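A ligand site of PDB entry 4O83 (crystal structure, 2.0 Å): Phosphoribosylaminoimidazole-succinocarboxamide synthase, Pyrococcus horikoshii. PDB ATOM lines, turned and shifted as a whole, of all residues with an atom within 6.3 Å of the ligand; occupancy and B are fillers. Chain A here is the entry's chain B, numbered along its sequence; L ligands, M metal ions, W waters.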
ATOM      1  N   ALA A  12       7.486 -21.350 -29.190  1.00  0.00           N
ATOM      2  CA  ALA A  12       8.531 -20.357 -28.852  1.00  0.00           C
ATOM      3  C   ALA A  12       8.589 -20.001 -27.349  1.00  0.00           C
ATOM      4  O   ALA A  12       9.535 -19.346 -26.894  1.00  0.00           O
ATOM      5  CB  ALA A  12       8.388 -19.108 -29.711  1.00  0.00           C
ATOM      6  N   LYS A  13       7.586 -20.431 -26.577  1.00  0.00           N
ATOM      7  CA  LYS A  13       7.639 -20.342 -25.114  1.00  0.00           C
ATOM      8  C   LYS A  13       7.296 -21.688 -24.471  1.00  0.00           C
ATOM      9  O   LYS A  13       6.514 -22.474 -25.020  1.00  0.00           O
ATOM     10  CB  LYS A  13       6.692 -19.260 -24.553  1.00  0.00           C
ATOM     11  CG  LYS A  13       6.965 -17.831 -25.017  1.00  0.00           C
ATOM     12  CD  LYS A  13       6.213 -16.793 -24.194  1.00  0.00           C
ATOM     13  CE  LYS A  13       4.691 -16.898 -24.283  1.00  0.00           C
ATOM     14  NZ  LYS A  13       4.114 -16.679 -25.644  1.00  0.00           N
ATOM     15  N   LYS A  14       7.881 -21.960 -23.308  1.00  0.00           N
ATOM     16  CA  LYS A  14       7.498 -23.117 -22.507  1.00  0.00           C
ATOM     17  C   LYS A  14       7.000 -22.650 -21.143  1.00  0.00           C
ATOM     18  O   LYS A  14       7.704 -21.903 -20.457  1.00  0.00           O
ATOM     19  CB  LYS A  14       8.659 -24.105 -22.360  1.00  0.00           C
ATOM     20  N   MET A  15       5.807 -23.088 -20.774  1.00  0.00           N
ATOM     21  CA  MET A  15       5.197 -22.739 -19.487  1.00  0.00           C
ATOM     22  C   MET A  15       5.359 -23.908 -18.570  1.00  0.00           C
ATOM     23  O   MET A  15       4.810 -24.985 -18.816  1.00  0.00           O
ATOM     24  CB  MET A  15       3.714 -22.395 -19.592  1.00  0.00           C
ATOM     25  CG  MET A  15       3.367 -21.460 -20.746  1.00  0.00           C
ATOM     26  SD  MET A  15       4.185 -19.664 -20.567  1.00  0.00           S
ATOM     27  CE  MET A  15       2.831 -18.885 -19.365  1.00  0.00           C
ATOM     28  N   LEU A  23       4.034 -19.752 -12.319  1.00  0.00           N
ATOM     29  CA  LEU A  23       4.704 -20.575 -13.299  1.00  0.00           C
ATOM     30  C   LEU A  23       5.898 -19.871 -13.926  1.00  0.00           C
ATOM     31  O   LEU A  23       6.104 -18.677 -13.740  1.00  0.00           O
ATOM     32  CB  LEU A  23       3.724 -21.108 -14.346  1.00  0.00           C
ATOM     33  CG  LEU A  23       2.958 -20.141 -15.231  1.00  0.00           C
ATOM     34  CD1 LEU A  23       3.767 -19.980 -16.496  1.00  0.00           C
ATOM     35  CD2 LEU A  23       1.591 -20.723 -15.560  1.00  0.00           C
ATOM     36  N   MET A  25       7.764 -18.903 -17.388  1.00  0.00           N
ATOM     37  CA  MET A  25       7.639 -18.696 -18.809  1.00  0.00           C
ATOM     38  C   MET A  25       9.044 -18.717 -19.357  1.00  0.00           C
ATOM     39  O   MET A  25       9.849 -17.825 -19.070  1.00  0.00           O
ATOM     40  CB  MET A  25       6.930 -17.360 -19.035  1.00  0.00           C
ATOM     41  CG  MET A  25       6.712 -17.046 -20.521  1.00  0.00           C
ATOM     42  SD  MET A  25       5.299 -15.677 -20.753  1.00  0.00           S
ATOM     43  CE  MET A  25       6.162 -14.178 -19.816  1.00  0.00           C
ATOM     44  N   HIS A  68       0.868 -10.197 -15.261  1.00  0.00           N
ATOM     45  CA  HIS A  68       1.211 -11.465 -14.636  1.00  0.00           C
ATOM     46  C   HIS A  68       2.670 -11.544 -14.223  1.00  0.00           C
ATOM     47  O   HIS A  68       3.083 -12.517 -13.589  1.00  0.00           O
ATOM     48  CB  HIS A  68       0.814 -12.634 -15.537  1.00  0.00           C
ATOM     49  CG  HIS A  68       1.678 -12.791 -16.759  1.00  0.00           C
ATOM     50  ND1 HIS A  68       1.825 -13.966 -17.388  1.00  0.00           N
ATOM     51  CD2 HIS A  68       2.438 -11.870 -17.489  1.00  0.00           C
ATOM     52  CE1 HIS A  68       2.627 -13.815 -18.454  1.00  0.00           C
ATOM     53  NE2 HIS A  68       3.003 -12.527 -18.520  1.00  0.00           N
ATOM     54  N   VAL A  80       5.869 -15.868 -13.609  1.00  0.00           N
ATOM     55  CA  VAL A  80       4.594 -15.177 -13.789  1.00  0.00           C
ATOM     56  C   VAL A  80       3.504 -15.843 -12.957  1.00  0.00           C
ATOM     57  O   VAL A  80       3.608 -17.027 -12.626  1.00  0.00           O
ATOM     58  CB  VAL A  80       4.175 -15.136 -15.265  1.00  0.00           C
ATOM     59  CG1 VAL A  80       5.159 -14.310 -16.085  1.00  0.00           C
ATOM     60  CG2 VAL A  80       4.047 -16.541 -15.847  1.00  0.00           C
ATOM     61  N   GLU A  81       2.487 -15.074 -12.596  1.00  0.00           N
ATOM     62  CA  GLU A  81       1.374 -15.616 -11.816  1.00  0.00           C
ATOM     63  C   GLU A  81       0.416 -16.382 -12.710  1.00  0.00           C
ATOM     64  O   GLU A  81       0.174 -15.983 -13.858  1.00  0.00           O
ATOM     65  CB  GLU A  81       0.659 -14.541 -10.991  1.00  0.00           C
ATOM     66  CG  GLU A  81      -0.161 -13.533 -11.752  1.00  0.00           C
ATOM     67  CD  GLU A  81      -0.996 -12.662 -10.827  1.00  0.00           C
ATOM     68  OE1 GLU A  81      -0.938 -11.416 -10.971  1.00  0.00           O
ATOM     69  OE2 GLU A  81      -1.677 -13.218  -9.939  1.00  0.00           O
ATOM     70  N   LYS A  82      -0.087 -17.500 -12.194  1.00  0.00           N
ATOM     71  CA  LYS A  82      -0.939 -18.380 -12.981  1.00  0.00           C
ATOM     72  C   LYS A  82      -2.326 -17.766 -13.054  1.00  0.00           C
ATOM     73  O   LYS A  82      -2.863 -17.273 -12.047  1.00  0.00           O
ATOM     74  CB  LYS A  82      -0.963 -19.807 -12.414  1.00  0.00           C
ATOM     75  CG  LYS A  82      -1.522 -20.852 -13.377  1.00  0.00           C
ATOM     76  CD  LYS A  82      -1.052 -22.265 -13.046  1.00  0.00           C
ATOM     77  CE  LYS A  82      -1.959 -22.946 -12.031  1.00  0.00           C
ATOM     78  NZ  LYS A  82      -1.416 -24.260 -11.568  1.00  0.00           N
ATOM     79  N   LEU A  83      -2.897 -17.773 -14.249  1.00  0.00           N
ATOM     80  CA  LEU A  83      -4.173 -17.135 -14.471  1.00  0.00           C
ATOM     81  C   LEU A  83      -5.146 -18.102 -15.102  1.00  0.00           C
ATOM     82  O   LEU A  83      -4.742 -19.056 -15.780  1.00  0.00           O
ATOM     83  CB  LEU A  83      -4.010 -15.890 -15.366  1.00  0.00           C
ATOM     84  CG  LEU A  83      -3.105 -14.773 -14.855  1.00  0.00           C
ATOM     85  CD1 LEU A  83      -2.884 -13.725 -15.950  1.00  0.00           C
ATOM     86  CD2 LEU A  83      -3.667 -14.127 -13.589  1.00  0.00           C
ATOM     87  N   ASP A  84      -6.423 -17.849 -14.852  1.00  0.00           N
ATOM     88  CA  ASP A  84      -7.507 -18.413 -15.622  1.00  0.00           C
ATOM     89  C   ASP A  84      -7.641 -17.589 -16.902  1.00  0.00           C
ATOM     90  O   ASP A  84      -8.189 -16.498 -16.866  1.00  0.00           O
ATOM     91  CB  ASP A  84      -8.786 -18.320 -14.783  1.00  0.00           C
ATOM     92  CG  ASP A  84      -9.983 -18.936 -15.468  1.00  0.00           C
ATOM     93  OD1 ASP A  84      -9.818 -19.980 -16.133  1.00  0.00           O
ATOM     94  OD2 ASP A  84     -11.098 -18.374 -15.331  1.00  0.00           O
ATOM     95  N   MET A  85      -7.116 -18.110 -18.023  1.00  0.00           N
ATOM     96  CA  MET A  85      -6.952 -17.307 -19.253  1.00  0.00           C
ATOM     97  C   MET A  85      -8.256 -17.121 -19.997  1.00  0.00           C
ATOM     98  O   MET A  85      -9.060 -18.054 -20.113  1.00  0.00           O
ATOM     99  CB  MET A  85      -5.968 -17.931 -20.242  1.00  0.00           C
ATOM    100  CG  MET A  85      -4.523 -18.056 -19.737  1.00  0.00           C
ATOM    101  SD  MET A  85      -3.784 -16.259 -19.415  1.00  0.00           S
ATOM    102  CE  MET A  85      -3.641 -15.689 -21.290  1.00  0.00           C
ATOM    103  N   TYR A  86      -8.458 -15.923 -20.534  1.00  0.00           N
ATOM    104  CA  TYR A  86      -9.536 -15.723 -21.497  1.00  0.00           C
ATOM    105  C   TYR A  86      -9.108 -16.335 -22.814  1.00  0.00           C
ATOM    106  O   TYR A  86      -7.954 -16.223 -23.190  1.00  0.00           O
ATOM    107  CB  TYR A  86      -9.859 -14.241 -21.669  1.00  0.00           C
ATOM    108  CG  TYR A  86     -10.554 -13.635 -20.490  1.00  0.00           C
ATOM    109  CD1 TYR A  86     -11.947 -13.750 -20.330  1.00  0.00           C
ATOM    110  CD2 TYR A  86      -9.830 -12.912 -19.534  1.00  0.00           C
ATOM    111  CE1 TYR A  86     -12.595 -13.172 -19.260  1.00  0.00           C
ATOM    112  CE2 TYR A  86     -10.471 -12.329 -18.450  1.00  0.00           C
ATOM    113  CZ  TYR A  86     -11.851 -12.462 -18.324  1.00  0.00           C
ATOM    114  OH  TYR A  86     -12.492 -11.897 -17.254  1.00  0.00           O
ATOM    115  N   GLU A  89      -7.131 -13.636 -28.286  1.00  0.00           N
ATOM    116  CA  GLU A  89      -6.022 -12.790 -28.693  1.00  0.00           C
ATOM    117  C   GLU A  89      -6.623 -11.412 -29.011  1.00  0.00           C
ATOM    118  O   GLU A  89      -7.482 -11.277 -29.887  1.00  0.00           O
ATOM    119  CB  GLU A  89      -5.257 -13.396 -29.875  1.00  0.00           C
ATOM    120  CG  GLU A  89      -4.780 -14.816 -29.607  1.00  0.00           C
ATOM    121  CD  GLU A  89      -3.650 -15.261 -30.524  1.00  0.00           C
ATOM    122  OE1 GLU A  89      -2.524 -14.763 -30.367  1.00  0.00           O
ATOM    123  OE2 GLU A  89      -3.894 -16.119 -31.396  1.00  0.00           O
ATOM    124  N   LYS A 122      -9.020 -17.499 -29.657  1.00  0.00           N
ATOM    125  CA  LYS A 122      -7.748 -18.207 -29.640  1.00  0.00           C
ATOM    126  C   LYS A 122      -8.031 -19.707 -29.814  1.00  0.00           C
ATOM    127  O   LYS A 122      -8.478 -20.371 -28.895  1.00  0.00           O
ATOM    128  CB  LYS A 122      -7.035 -17.922 -28.318  1.00  0.00           C
ATOM    129  CG  LYS A 122      -5.575 -18.299 -28.285  1.00  0.00           C
ATOM    130  CD  LYS A 122      -4.948 -17.907 -26.949  1.00  0.00           C
ATOM    131  CE  LYS A 122      -3.545 -18.476 -26.804  1.00  0.00           C
ATOM    132  NZ  LYS A 122      -2.625 -18.028 -27.893  1.00  0.00           N
ATOM    133  N   ASP A 124      -6.294 -22.724 -32.533  1.00  0.00           N
ATOM    134  CA  ASP A 124      -5.400 -23.103 -33.637  1.00  0.00           C
ATOM    135  C   ASP A 124      -6.142 -23.773 -34.786  1.00  0.00           C
ATOM    136  O   ASP A 124      -5.870 -23.478 -35.962  1.00  0.00           O
ATOM    137  CB  ASP A 124      -4.287 -24.045 -33.160  1.00  0.00           C
ATOM    138  CG  ASP A 124      -3.345 -23.381 -32.167  1.00  0.00           C
ATOM    139  OD1 ASP A 124      -2.986 -22.208 -32.375  1.00  0.00           O
ATOM    140  OD2 ASP A 124      -2.942 -24.055 -31.189  1.00  0.00           O
ATOM    141  N   LYS A 175      -0.474  -7.790 -30.222  1.00  0.00           N
ATOM    142  CA  LYS A 175      -1.433  -8.764 -29.711  1.00  0.00           C
ATOM    143  C   LYS A 175      -1.242  -8.895 -28.200  1.00  0.00           C
ATOM    144  O   LYS A 175      -0.122  -8.997 -27.718  1.00  0.00           O
ATOM    145  CB  LYS A 175      -1.245 -10.099 -30.435  1.00  0.00           C
ATOM    146  CG  LYS A 175      -2.204 -11.225 -29.992  1.00  0.00           C
ATOM    147  CD  LYS A 175      -1.688 -12.035 -28.807  1.00  0.00           C
ATOM    148  CE  LYS A 175      -0.398 -12.816 -29.142  1.00  0.00           C
ATOM    149  NZ  LYS A 175       0.174 -13.487 -27.933  1.00  0.00           N
ATOM    150  N   GLU A 177      -2.858 -10.852 -24.499  1.00  0.00           N
ATOM    151  CA  GLU A 177      -3.705 -11.870 -23.880  1.00  0.00           C
ATOM    152  C   GLU A 177      -3.957 -11.517 -22.412  1.00  0.00           C
ATOM    153  O   GLU A 177      -3.123 -10.851 -21.767  1.00  0.00           O
ATOM    154  CB  GLU A 177      -3.048 -13.238 -24.011  1.00  0.00           C
ATOM    155  CG  GLU A 177      -2.660 -13.569 -25.448  1.00  0.00           C
ATOM    156  CD  GLU A 177      -2.319 -15.020 -25.679  1.00  0.00           C
ATOM    157  OE1 GLU A 177      -2.532 -15.843 -24.770  1.00  0.00           O
ATOM    158  OE2 GLU A 177      -1.834 -15.334 -26.776  1.00  0.00           O
ATOM    159  N   LEU A 188      -3.136  -8.674 -17.438  1.00  0.00           N
ATOM    160  CA  LEU A 188      -2.404  -8.819 -18.691  1.00  0.00           C
ATOM    161  C   LEU A 188      -1.343  -9.909 -18.599  1.00  0.00           C
ATOM    162  O   LEU A 188      -0.535  -9.940 -17.671  1.00  0.00           O
ATOM    163  CB  LEU A 188      -1.787  -7.490 -19.095  1.00  0.00           C
ATOM    164  CG  LEU A 188      -0.920  -7.467 -20.361  1.00  0.00           C
ATOM    165  CD1 LEU A 188      -1.798  -7.640 -21.603  1.00  0.00           C
ATOM    166  CD2 LEU A 188      -0.114  -6.182 -20.419  1.00  0.00           C
ATOM    167  N   ALA A 189      -1.339 -10.800 -19.589  1.00  0.00           N
ATOM    168  CA  ALA A 189      -0.528 -11.996 -19.534  1.00  0.00           C
ATOM    169  C   ALA A 189       0.373 -12.173 -20.775  1.00  0.00           C
ATOM    170  O   ALA A 189       0.679 -11.212 -21.487  1.00  0.00           O
ATOM    171  CB  ALA A 189      -1.422 -13.203 -19.349  1.00  0.00           C
ATOM    172  N   ASP A 190       0.773 -13.426 -21.003  1.00  0.00           N
ATOM    173  CA  ASP A 190       1.606 -13.858 -22.125  1.00  0.00           C
ATOM    174  C   ASP A 190       2.897 -13.039 -22.236  1.00  0.00           C
ATOM    175  O   ASP A 190       3.588 -12.840 -21.234  1.00  0.00           O
ATOM    176  CB  ASP A 190       0.803 -13.834 -23.428  1.00  0.00           C
ATOM    177  CG  ASP A 190       1.372 -14.753 -24.485  1.00  0.00           C
ATOM    178  OD1 ASP A 190       1.748 -14.269 -25.563  1.00  0.00           O
ATOM    179  OD2 ASP A 190       1.464 -15.971 -24.217  1.00  0.00           O
ATOM    180  N   GLU A 191       3.223 -12.575 -23.445  1.00  0.00           N
ATOM    181  CA  GLU A 191       4.471 -11.827 -23.665  1.00  0.00           C
ATOM    182  C   GLU A 191       4.186 -10.548 -24.400  1.00  0.00           C
ATOM    183  O   GLU A 191       3.119 -10.388 -24.978  1.00  0.00           O
ATOM    184  CB  GLU A 191       5.469 -12.672 -24.488  1.00  0.00           C
ATOM    185  CG  GLU A 191       5.032 -12.901 -25.933  1.00  0.00           C
ATOM    186  CD  GLU A 191       6.008 -13.733 -26.721  1.00  0.00           C
ATOM    187  OE1 GLU A 191       7.137 -13.253 -26.989  1.00  0.00           O
ATOM    188  OE2 GLU A 191       5.644 -14.856 -27.096  1.00  0.00           O
HETATM  189  P1  LIG L   1       0.731 -20.863 -28.150  1.00  0.00           P
HETATM  190  O1  LIG L   1      -0.200 -19.674 -28.092  1.00  0.00           O
HETATM  191  O2  LIG L   1       1.824 -20.755 -29.196  1.00  0.00           O
HETATM  192  O3  LIG L   1       0.015 -22.197 -28.142  1.00  0.00           O
HETATM  193  P2  LIG L   1       2.927 -20.282 -26.389  1.00  0.00           P
HETATM  194  O4  LIG L   1       3.829 -21.414 -25.953  1.00  0.00           O
HETATM  195  O5  LIG L   1       3.385 -19.360 -27.494  1.00  0.00           O
HETATM  196  O6  LIG L   1       1.474 -20.915 -26.723  1.00  0.00           O
HETATM  197  O7  LIG L   1       2.554 -19.386 -25.105  1.00  0.00           O
HETATM  198  C1  LIG L   1       2.336 -19.963 -23.817  1.00  0.00           C
HETATM  199  C2  LIG L   1       0.854 -20.238 -23.519  1.00  0.00           C
HETATM  200  O8  LIG L   1       0.555 -19.933 -22.154  1.00  0.00           O
HETATM  201  C3  LIG L   1      -0.146 -19.453 -24.348  1.00  0.00           C
HETATM  202  O9  LIG L   1      -1.133 -20.371 -24.824  1.00  0.00           O
HETATM  203  C4  LIG L   1      -0.799 -18.458 -23.397  1.00  0.00           C
HETATM  204  O10 LIG L   1      -2.166 -18.287 -23.719  1.00  0.00           O
HETATM  205  C5  LIG L   1      -0.622 -19.122 -22.045  1.00  0.00           C
HETATM  206  N1  LIG L   1      -0.344 -18.167 -20.944  1.00  0.00           N
HETATM  207  C6  LIG L   1       0.388 -17.050 -21.041  1.00  0.00           C
HETATM  208  N2  LIG L   1       0.475 -16.432 -19.850  1.00  0.00           N
HETATM  209  C7  LIG L   1      -0.202 -17.156 -18.954  1.00  0.00           C
HETATM  210  C8  LIG L   1      -0.514 -17.076 -17.495  1.00  0.00           C
HETATM  211  N3  LIG L   1      -0.074 -16.045 -16.738  1.00  0.00           N
HETATM  212  N4  LIG L   1      -1.269 -18.045 -16.955  1.00  0.00           N
HETATM  213  C9  LIG L   1      -1.720 -19.081 -17.684  1.00  0.00           C
HETATM  214  N5  LIG L   1      -1.480 -19.229 -19.005  1.00  0.00           N
HETATM  215  C10 LIG L   1      -0.749 -18.306 -19.681  1.00  0.00           C
HETATM  216 CD    CD M   1       1.542 -17.549 -28.136  1.00  0.00          CD
HETATM  217 CD    CD M   2      -2.905 -18.087 -31.966  1.00  0.00          CD
HETATM  218  O   HOH W   1      -5.185 -17.004 -24.182  1.00  0.00           O
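The backbone NH (N) of His 68 is in hydrogen-bond range of the backbone carbonyl oxygen (O) of Leu 188, at 2.8 Å. NZ of Lys 13 is in salt-bridge range of OD2 of Asp 190 (3.1 Å). NZ of Lys 122 lies within salt-bridge range of OE2 of Glu 177 (3.0 Å). The side-chain carboxylate (OD1) of Asp 190 lies within salt-bridge range of the side-chain amino group (NZ) of Lys 175 (3.0 Å). The backbone carbonyl oxygen (O) of Glu 177 lies within hydrogen-bond range of the backbone NH (N) of Ala 189. A ring nitrogen (NE2) of His 68 lies within hydrogen-bond range of the backbone carbonyl oxygen of Asp 190 (2.8 Å). The backbone carbonyl oxygen (O) of His 68 sits at hydrogen-bond distance from the backbone NH (N) of Glu 81, 2.8 Å away. NZ of Lys 13 lies within salt-bridge range of OE2 of Glu 191, 2.8 Å away.
SD of Met 85 sits close to N5 of the ligand (3.8 Å). Met 15 touches the ligand (CE to N2, 3.4 Å). CB of Ala 189 touches N2 of the ligand, at 3.8 Å. Hydrophobic or aromatic side chains within 4 Å of the ligand: Met 15, His 68, Leu 83, Met 85 and Ala 189. Within 4 Å of the ligand: Lys 13, Met 15, His 68, Glu 81, Leu 83, Met 85, Lys 122, Glu 177, Ala 189 and Asp 190.
Water W1 lies within hydrogen-bond range of the side-chain carboxylate (OE1) of Glu 177 (3.0 Å), the backbone carbonyl oxygen (O) of Tyr 86 (3.0 Å) and an oxygen (O10) of the ligand (3.3 Å).
A nitrogen (N4) of the ligand lies within hydrogen-bond range of the backbone NH of Leu 83 (3.2 Å). The backbone carbonyl oxygen (O) of Glu 81 lies within hydrogen-bond range of a nitrogen (N3) of the ligand (2.9 Å). OE1 of Glu 177 lies within hydrogen-bond range of O10 of the ligand, at 2.7 Å. The backbone carbonyl oxygen (O) of Lys 13 lies close to an oxygen (O4) of the ligand, 3.0 Å away. A nitrogen (N2) of the ligand lies within hydrogen-bond range of the backbone NH (N) of Asp 190, 3.2 Å away. A ring nitrogen (ND1) of His 68 is in hydrogen-bond range of a nitrogen (N3) of the ligand, at 2.9 Å. The side-chain amino group (NZ) of Lys 122 is in salt-bridge range of an oxygen (O1) of the ligand. An oxygen (O5) of the ligand lies within salt-bridge range of the side-chain amino group (NZ) of Lys 13, at 3.3 Å.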
